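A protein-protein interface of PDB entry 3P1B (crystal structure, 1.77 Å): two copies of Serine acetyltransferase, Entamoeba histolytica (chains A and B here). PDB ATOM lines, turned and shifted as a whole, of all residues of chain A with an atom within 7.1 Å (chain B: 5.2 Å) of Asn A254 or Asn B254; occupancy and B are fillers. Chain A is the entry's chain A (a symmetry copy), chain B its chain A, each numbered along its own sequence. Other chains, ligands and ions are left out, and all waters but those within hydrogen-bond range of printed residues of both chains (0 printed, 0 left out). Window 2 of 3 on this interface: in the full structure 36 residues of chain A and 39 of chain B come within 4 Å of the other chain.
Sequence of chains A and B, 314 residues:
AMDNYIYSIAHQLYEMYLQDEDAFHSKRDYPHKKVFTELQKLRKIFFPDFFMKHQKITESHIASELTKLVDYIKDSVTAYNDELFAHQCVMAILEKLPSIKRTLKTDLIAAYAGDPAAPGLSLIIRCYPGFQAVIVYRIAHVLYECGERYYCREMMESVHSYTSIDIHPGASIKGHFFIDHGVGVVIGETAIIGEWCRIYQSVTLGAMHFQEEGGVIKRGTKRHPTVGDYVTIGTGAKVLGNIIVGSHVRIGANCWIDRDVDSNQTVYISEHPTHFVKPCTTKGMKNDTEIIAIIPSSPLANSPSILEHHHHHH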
ATOM      1  N   GLN A 201       1.455  -5.570  28.909  1.00  0.00           N
ATOM      2  CA  GLN A 201       2.373  -4.622  28.298  1.00  0.00           C
ATOM      3  C   GLN A 201       3.690  -5.277  27.797  1.00  0.00           C
ATOM      4  O   GLN A 201       4.177  -6.260  28.375  1.00  0.00           O
ATOM      5  CB  GLN A 201       2.702  -3.447  29.262  1.00  0.00           C
ATOM      6  CG  GLN A 201       3.435  -3.907  30.573  1.00  0.00           C
ATOM      7  CD  GLN A 201       2.473  -4.328  31.687  1.00  0.00           C
ATOM      8  OE1 GLN A 201       1.349  -4.781  31.444  1.00  0.00           O
ATOM      9  NE2 GLN A 201       2.935  -4.176  32.941  1.00  0.00           N
ATOM     10  N   SER A 202       4.206  -4.736  26.705  1.00  0.00           N
ATOM     11  CA  SER A 202       5.522  -5.122  26.176  1.00  0.00           C
ATOM     12  C   SER A 202       5.678  -6.554  25.628  1.00  0.00           C
ATOM     13  O   SER A 202       6.788  -7.064  25.418  1.00  0.00           O
ATOM     14  CB  SER A 202       6.600  -4.790  27.210  1.00  0.00           C
ATOM     15  OG  SER A 202       6.939  -3.430  27.096  1.00  0.00           O
ATOM     16  N   MET A 208      10.707 -10.683  13.714  1.00  0.00           N
ATOM     17  CA  MET A 208      11.860  -9.788  13.442  1.00  0.00           C
ATOM     18  C   MET A 208      12.531 -10.201  12.134  1.00  0.00           C
ATOM     19  O   MET A 208      12.314 -11.317  11.674  1.00  0.00           O
ATOM     20  CB  MET A 208      12.896  -9.986  14.531  1.00  0.00           C
ATOM     21  CG  MET A 208      12.906  -8.960  15.637  1.00  0.00           C
ATOM     22  SD  MET A 208      14.105  -9.629  16.790  1.00  0.00           S
ATOM     23  CE  MET A 208      15.061 -10.775  15.789  1.00  0.00           C
ATOM     24  N   GLY A 234       3.249 -12.939  29.834  1.00  0.00           N
ATOM     25  CA  GLY A 234       3.698 -12.019  30.857  1.00  0.00           C
ATOM     26  C   GLY A 234       4.428 -10.834  30.266  1.00  0.00           C
ATOM     27  O   GLY A 234       4.981 -10.918  29.135  1.00  0.00           O
ATOM     28  N   THR A 235       4.399  -9.749  31.038  1.00  0.00           N
ATOM     29  CA  THR A 235       5.013  -8.473  30.739  1.00  0.00           C
ATOM     30  C   THR A 235       6.406  -8.662  30.070  1.00  0.00           C
ATOM     31  O   THR A 235       7.299  -9.350  30.611  1.00  0.00           O
ATOM     32  CB  THR A 235       5.139  -7.688  32.092  1.00  0.00           C
ATOM     33  OG1 THR A 235       6.031  -8.424  32.954  1.00  0.00           O
ATOM     34  CG2 THR A 235       3.783  -7.626  32.787  1.00  0.00           C
ATOM     35  N   GLY A 236       6.592  -8.124  28.868  1.00  0.00           N
ATOM     36  CA  GLY A 236       7.949  -8.144  28.223  1.00  0.00           C
ATOM     37  C   GLY A 236       8.337  -9.323  27.326  1.00  0.00           C
ATOM     38  O   GLY A 236       9.380  -9.284  26.608  1.00  0.00           O
ATOM     39  N   ALA A 237       7.533 -10.390  27.371  1.00  0.00           N
ATOM     40  CA  ALA A 237       7.775 -11.591  26.563  1.00  0.00           C
ATOM     41  C   ALA A 237       7.734 -11.311  25.051  1.00  0.00           C
ATOM     42  O   ALA A 237       6.819 -10.660  24.574  1.00  0.00           O
ATOM     43  CB  ALA A 237       6.779 -12.713  26.942  1.00  0.00           C
ATOM     44  N   LYS A 238       8.710 -11.845  24.304  1.00  0.00           N
ATOM     45  CA  LYS A 238       8.757 -11.654  22.862  1.00  0.00           C
ATOM     46  C   LYS A 238       8.640 -13.027  22.252  1.00  0.00           C
ATOM     47  O   LYS A 238       9.553 -13.825  22.383  1.00  0.00           O
ATOM     48  CB  LYS A 238      10.085 -11.003  22.434  1.00  0.00           C
ATOM     49  CG  LYS A 238      10.479  -9.736  23.221  1.00  0.00           C
ATOM     50  CD  LYS A 238       9.511  -8.586  22.926  1.00  0.00           C
ATOM     51  CE  LYS A 238       9.992  -7.267  23.501  1.00  0.00           C
ATOM     52  NZ  LYS A 238       9.674  -7.162  24.918  1.00  0.00           N
ATOM     53  N   ILE A 251       3.379 -17.816  29.995  1.00  0.00           N
ATOM     54  CA  ILE A 251       4.732 -17.448  29.643  1.00  0.00           C
ATOM     55  C   ILE A 251       5.178 -16.352  30.607  1.00  0.00           C
ATOM     56  O   ILE A 251       4.454 -15.401  30.841  1.00  0.00           O
ATOM     57  CB  ILE A 251       4.788 -16.922  28.192  1.00  0.00           C
ATOM     58  CG1 ILE A 251       4.294 -18.001  27.215  1.00  0.00           C
ATOM     59  CG2 ILE A 251       6.216 -16.464  27.859  1.00  0.00           C
ATOM     60  CD1 ILE A 251       3.772 -17.494  25.849  1.00  0.00           C
ATOM     61  N   GLY A 252       6.374 -16.496  31.150  1.00  0.00           N
ATOM     62  CA  GLY A 252       6.942 -15.537  32.098  1.00  0.00           C
ATOM     63  C   GLY A 252       7.278 -14.153  31.556  1.00  0.00           C
ATOM     64  O   GLY A 252       7.281 -13.897  30.327  1.00  0.00           O
ATOM     65  N   ALA A 253       7.565 -13.246  32.484  1.00  0.00           N
ATOM     66  CA  ALA A 253       8.003 -11.891  32.150  1.00  0.00           C
ATOM     67  C   ALA A 253       9.369 -11.893  31.400  1.00  0.00           C
ATOM     68  O   ALA A 253      10.259 -12.690  31.699  1.00  0.00           O
ATOM     69  CB  ALA A 253       8.034 -11.000  33.428  1.00  0.00           C
ATOM     70  N   ASN A 254       9.513 -11.047  30.381  1.00  0.00           N
ATOM     71  CA  ASN A 254      10.769 -10.939  29.639  1.00  0.00           C
ATOM     72  C   ASN A 254      11.283 -12.212  28.919  1.00  0.00           C
ATOM     73  O   ASN A 254      12.419 -12.256  28.435  1.00  0.00           O
ATOM     74  CB  ASN A 254      11.850 -10.317  30.526  1.00  0.00           C
ATOM     75  CG  ASN A 254      11.608  -8.843  30.790  1.00  0.00           C
ATOM     76  OD1 ASN A 254      10.642  -8.227  30.274  1.00  0.00           O
ATOM     77  ND2 ASN A 254      12.498  -8.247  31.581  1.00  0.00           N
ATOM     78  N   CYS A 255      10.441 -13.228  28.828  1.00  0.00           N
ATOM     79  CA  CYS A 255      10.795 -14.443  28.084  1.00  0.00           C
ATOM     80  C   CYS A 255      10.959 -14.172  26.582  1.00  0.00           C
ATOM     81  O   CYS A 255      10.232 -13.399  25.995  1.00  0.00           O
ATOM     82  CB  CYS A 255       9.783 -15.565  28.335  1.00  0.00           C
ATOM     83  SG  CYS A 255      10.119 -16.568  29.851  1.00  0.00           S
ATOM     84  N   TRP A 256      11.938 -14.822  25.976  1.00  0.00           N
ATOM     85  CA  TRP A 256      12.192 -14.751  24.550  1.00  0.00           C
ATOM     86  C   TRP A 256      11.831 -16.129  23.966  1.00  0.00           C
ATOM     87  O   TRP A 256      12.555 -17.083  24.191  1.00  0.00           O
ATOM     88  CB  TRP A 256      13.677 -14.379  24.394  1.00  0.00           C
ATOM     89  CG  TRP A 256      14.415 -14.565  23.077  1.00  0.00           C
ATOM     90  CD1 TRP A 256      15.785 -14.775  22.946  1.00  0.00           C
ATOM     91  CD2 TRP A 256      13.874 -14.591  21.749  1.00  0.00           C
ATOM     92  NE1 TRP A 256      16.129 -14.915  21.629  1.00  0.00           N
ATOM     93  CE2 TRP A 256      15.005 -14.675  20.834  1.00  0.00           C
ATOM     94  CE3 TRP A 256      12.609 -14.355  21.207  1.00  0.00           C
ATOM     95  CZ2 TRP A 256      14.816 -14.821  19.437  1.00  0.00           C
ATOM     96  CZ3 TRP A 256      12.448 -14.416  19.835  1.00  0.00           C
ATOM     97  CH2 TRP A 256      13.544 -14.613  18.960  1.00  0.00           C
ATOM     98  N   ILE A 257      10.676 -16.223  23.282  1.00  0.00           N
ATOM     99  CA  ILE A 257      10.150 -17.498  22.754  1.00  0.00           C
ATOM    100  C   ILE A 257      10.357 -17.582  21.236  1.00  0.00           C
ATOM    101  O   ILE A 257       9.820 -16.770  20.462  1.00  0.00           O
ATOM    102  CB  ILE A 257       8.625 -17.736  23.096  1.00  0.00           C
ATOM    103  CG1 ILE A 257       8.286 -17.427  24.567  1.00  0.00           C
ATOM    104  CG2 ILE A 257       8.195 -19.178  22.742  1.00  0.00           C
ATOM    105  CD1 ILE A 257       8.957 -18.321  25.601  1.00  0.00           C
ATOM    106  N   ILE A 269      12.353 -18.395  33.583  1.00  0.00           N
ATOM    107  CA  ILE A 269      13.748 -18.775  33.896  1.00  0.00           C
ATOM    108  C   ILE A 269      14.216 -18.248  35.271  1.00  0.00           C
ATOM    109  O   ILE A 269      13.448 -17.585  36.006  1.00  0.00           O
ATOM    110  CB  ILE A 269      14.755 -18.498  32.692  1.00  0.00           C
ATOM    111  CG1 ILE A 269      15.853 -19.586  32.612  1.00  0.00           C
ATOM    112  CG2 ILE A 269      15.310 -17.044  32.708  1.00  0.00           C
ATOM    113  CD1 ILE A 269      15.375 -20.945  32.081  1.00  0.00           C
ATOM    114  N   GLY B 234      16.962  -6.227  17.680  1.00  0.00           N
ATOM    115  CA  GLY B 234      15.733  -6.966  17.886  1.00  0.00           C
ATOM    116  C   GLY B 234      14.923  -6.400  19.031  1.00  0.00           C
ATOM    117  O   GLY B 234      15.482  -5.736  19.947  1.00  0.00           O
ATOM    118  N   THR B 235      13.621  -6.660  18.944  1.00  0.00           N
ATOM    119  CA  THR B 235      12.604  -6.255  19.891  1.00  0.00           C
ATOM    120  C   THR B 235      13.117  -6.383  21.355  1.00  0.00           C
ATOM    121  O   THR B 235      13.576  -7.462  21.792  1.00  0.00           O
ATOM    122  CB  THR B 235      11.351  -7.168  19.651  1.00  0.00           C
ATOM    123  OG1 THR B 235      11.726  -8.528  19.951  1.00  0.00           O
ATOM    124  CG2 THR B 235      10.946  -7.121  18.181  1.00  0.00           C
ATOM    125  N   GLY B 236      13.115  -5.287  22.108  1.00  0.00           N
ATOM    126  CA  GLY B 236      13.462  -5.361  23.569  1.00  0.00           C
ATOM    127  C   GLY B 236      14.919  -5.188  24.005  1.00  0.00           C
ATOM    128  O   GLY B 236      15.225  -5.042  25.225  1.00  0.00           O
ATOM    129  N   ALA B 237      15.836  -5.228  23.033  1.00  0.00           N
ATOM    130  CA  ALA B 237      17.270  -5.071  23.298  1.00  0.00           C
ATOM    131  C   ALA B 237      17.617  -3.704  23.912  1.00  0.00           C
ATOM    132  O   ALA B 237      17.165  -2.681  23.423  1.00  0.00           O
ATOM    133  CB  ALA B 237      18.094  -5.321  22.013  1.00  0.00           C
ATOM    134  N   GLY B 252      19.852  -9.909  19.177  1.00  0.00           N
ATOM    135  CA  GLY B 252      18.623 -10.625  19.528  1.00  0.00           C
ATOM    136  C   GLY B 252      17.593  -9.857  20.345  1.00  0.00           C
ATOM    137  O   GLY B 252      17.849  -8.752  20.882  1.00  0.00           O
ATOM    138  N   ALA B 253      16.405 -10.449  20.440  1.00  0.00           N
ATOM    139  CA  ALA B 253      15.321  -9.909  21.260  1.00  0.00           C
ATOM    140  C   ALA B 253      15.695  -9.894  22.774  1.00  0.00           C
ATOM    141  O   ALA B 253      16.350 -10.807  23.278  1.00  0.00           O
ATOM    142  CB  ALA B 253      13.997 -10.682  20.987  1.00  0.00           C
ATOM    143  N   ASN B 254      15.335  -8.827  23.487  1.00  0.00           N
ATOM    144  CA  ASN B 254      15.599  -8.734  24.922  1.00  0.00           C
ATOM    145  C   ASN B 254      17.078  -8.794  25.381  1.00  0.00           C
ATOM    146  O   ASN B 254      17.371  -8.912  26.576  1.00  0.00           O
ATOM    147  CB  ASN B 254      14.731  -9.740  25.680  1.00  0.00           C
ATOM    148  CG  ASN B 254      13.263  -9.355  25.687  1.00  0.00           C
ATOM    149  OD1 ASN B 254      12.856  -8.288  25.160  1.00  0.00           O
ATOM    150  ND2 ASN B 254      12.448 -10.205  26.307  1.00  0.00           N
ATOM    151  N   CYS B 255      18.001  -8.688  24.439  1.00  0.00           N
ATOM    152  CA  CYS B 255      19.428  -8.637  24.777  1.00  0.00           C
ATOM    153  C   CYS B 255      19.790  -7.373  25.568  1.00  0.00           C
ATOM    154  O   CYS B 255      19.279  -6.301  25.317  1.00  0.00           O
ATOM    155  CB  CYS B 255      20.302  -8.775  23.526  1.00  0.00           C
ATOM    156  SG  CYS B 255      20.631 -10.521  23.015  1.00  0.00           S
ATOM    157  N   TRP B 256      20.677  -7.525  26.536  1.00  0.00           N
ATOM    158  CA  TRP B 256      21.196  -6.431  27.335  1.00  0.00           C
ATOM    159  C   TRP B 256      22.673  -6.250  26.934  1.00  0.00           C
ATOM    160  O   TRP B 256      23.492  -7.082  27.284  1.00  0.00           O
ATOM    161  CB  TRP B 256      20.995  -6.836  28.805  1.00  0.00           C
ATOM    162  CG  TRP B 256      21.731  -6.134  29.936  1.00  0.00           C
ATOM    163  CD1 TRP B 256      22.045  -6.705  31.167  1.00  0.00           C
ATOM    164  CD2 TRP B 256      22.257  -4.800  29.964  1.00  0.00           C
ATOM    165  NE1 TRP B 256      22.719  -5.813  31.956  1.00  0.00           N
ATOM    166  CE2 TRP B 256      22.759  -4.573  31.312  1.00  0.00           C
ATOM    167  CE3 TRP B 256      22.193  -3.709  29.096  1.00  0.00           C
ATOM    168  CZ2 TRP B 256      23.442  -3.379  31.655  1.00  0.00           C
ATOM    169  CZ3 TRP B 256      22.789  -2.519  29.473  1.00  0.00           C
ATOM    170  CH2 TRP B 256      23.376  -2.347  30.750  1.00  0.00           C
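N of Thr B235 is in hydrogen-bond range of SD of Met A208 (3.7 Å).
The side-chain amide nitrogen (ND2) of Asn B254 lies within hydrogen-bond range of the backbone carbonyl oxygen (O) of Gly A236 (3.2 Å).
The side-chain amino group of Lys A238 is in hydrogen-bond range of the side-chain amide oxygen of Asn B254 (3.4 Å).
The side-chain amide nitrogen (ND2) of Asn B254 sits at hydrogen-bond distance from the backbone carbonyl oxygen (O) of Asn A254, 3.0 Å away.
The backbone carbonyl oxygen (O) of Thr B235 lies within hydrogen-bond range of the backbone NH (N) of Asn B254 (2.8 Å).
N of Gly A236 sits at hydrogen-bond distance from O of Gln A201.
O of Ser A202 sits at hydrogen-bond distance from NZ of Lys A238, 2.9 Å away.
NZ of Lys A238 is in hydrogen-bond range of O of Gly A236.
The backbone NH (N) of Lys A238 is in hydrogen-bond range of the backbone carbonyl oxygen (O) of Cys A255, 2.8 Å away.
The backbone carbonyl oxygen of Lys A238 lies within hydrogen-bond range of the backbone NH of Ile A257 (2.8 Å).
Printed residues of chain B that touch a printed residue of chain A: Gly B234, Thr B235, Gly B236, Ala B253 and Asn B254.
Hydrophobic or aromatic side chains of chain B that line the printed part of chain A: Ala B253.
Of the 16 printed residues of chain A, 6 touch a printed residue of chain B.
Hydrophobic or aromatic side chains of chain A that line the printed part of chain B: Met A208 and Trp A256.
Among the printed residues, 9 pairs touch across the chains.
Among the printed residues, no Asp or Glu carboxylate lies within 4 Å of a Lys or Arg side-chain nitrogen of the other chain.
Gly A236 touches Asn B254, but with the chains exchanged Asn A254 does not touch Gly B236 (7.5 Å).
Asn A254 touches its own counterpart, Asn B254.
Cys A255 touches Asn B254, but with the chains exchanged Asn A254 does not touch Cys B255 (7.7 Å).
Trp A256 touches Ala B253, but with the chains exchanged Ala A253 does not touch Trp B256 (12.6 Å).
Among the printed residues, pairs that only touch across the chains: Met A208 with Gly B234 (3.3 Å), Lys A238 with Thr B235 (3.7 Å), Lys A238 with Gly B236 (3.95 Å), Cys A255 with Asn B254 (3.9 Å) and Trp A256 with Ala B253 (3.9 Å).
Asn A254 touches just one residue of chain B: Asn B254 (3.0 Å).
Of the printed residues of chain A, Thr B235 touches Met A208 (3.7 Å) and Lys A238 (3.7 Å).
Of the printed residues of chain A, Gly B236 touches Lys A238.
Printed residues of chain B within 4 Å of Lys A238: Thr B235 (3.7 Å), Gly B236 (3.95 Å) and Asn B254 (3.4 Å).
Printed residues of chain A within 4 Å of Gly B234: Met A208.
The nearest printed residue of chain B that does not touch Asn A254 is Ala B253 (6.6 Å).
The nearest residue of chain A that does not touch Asn B254 is Trp A256 (4.7 Å).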
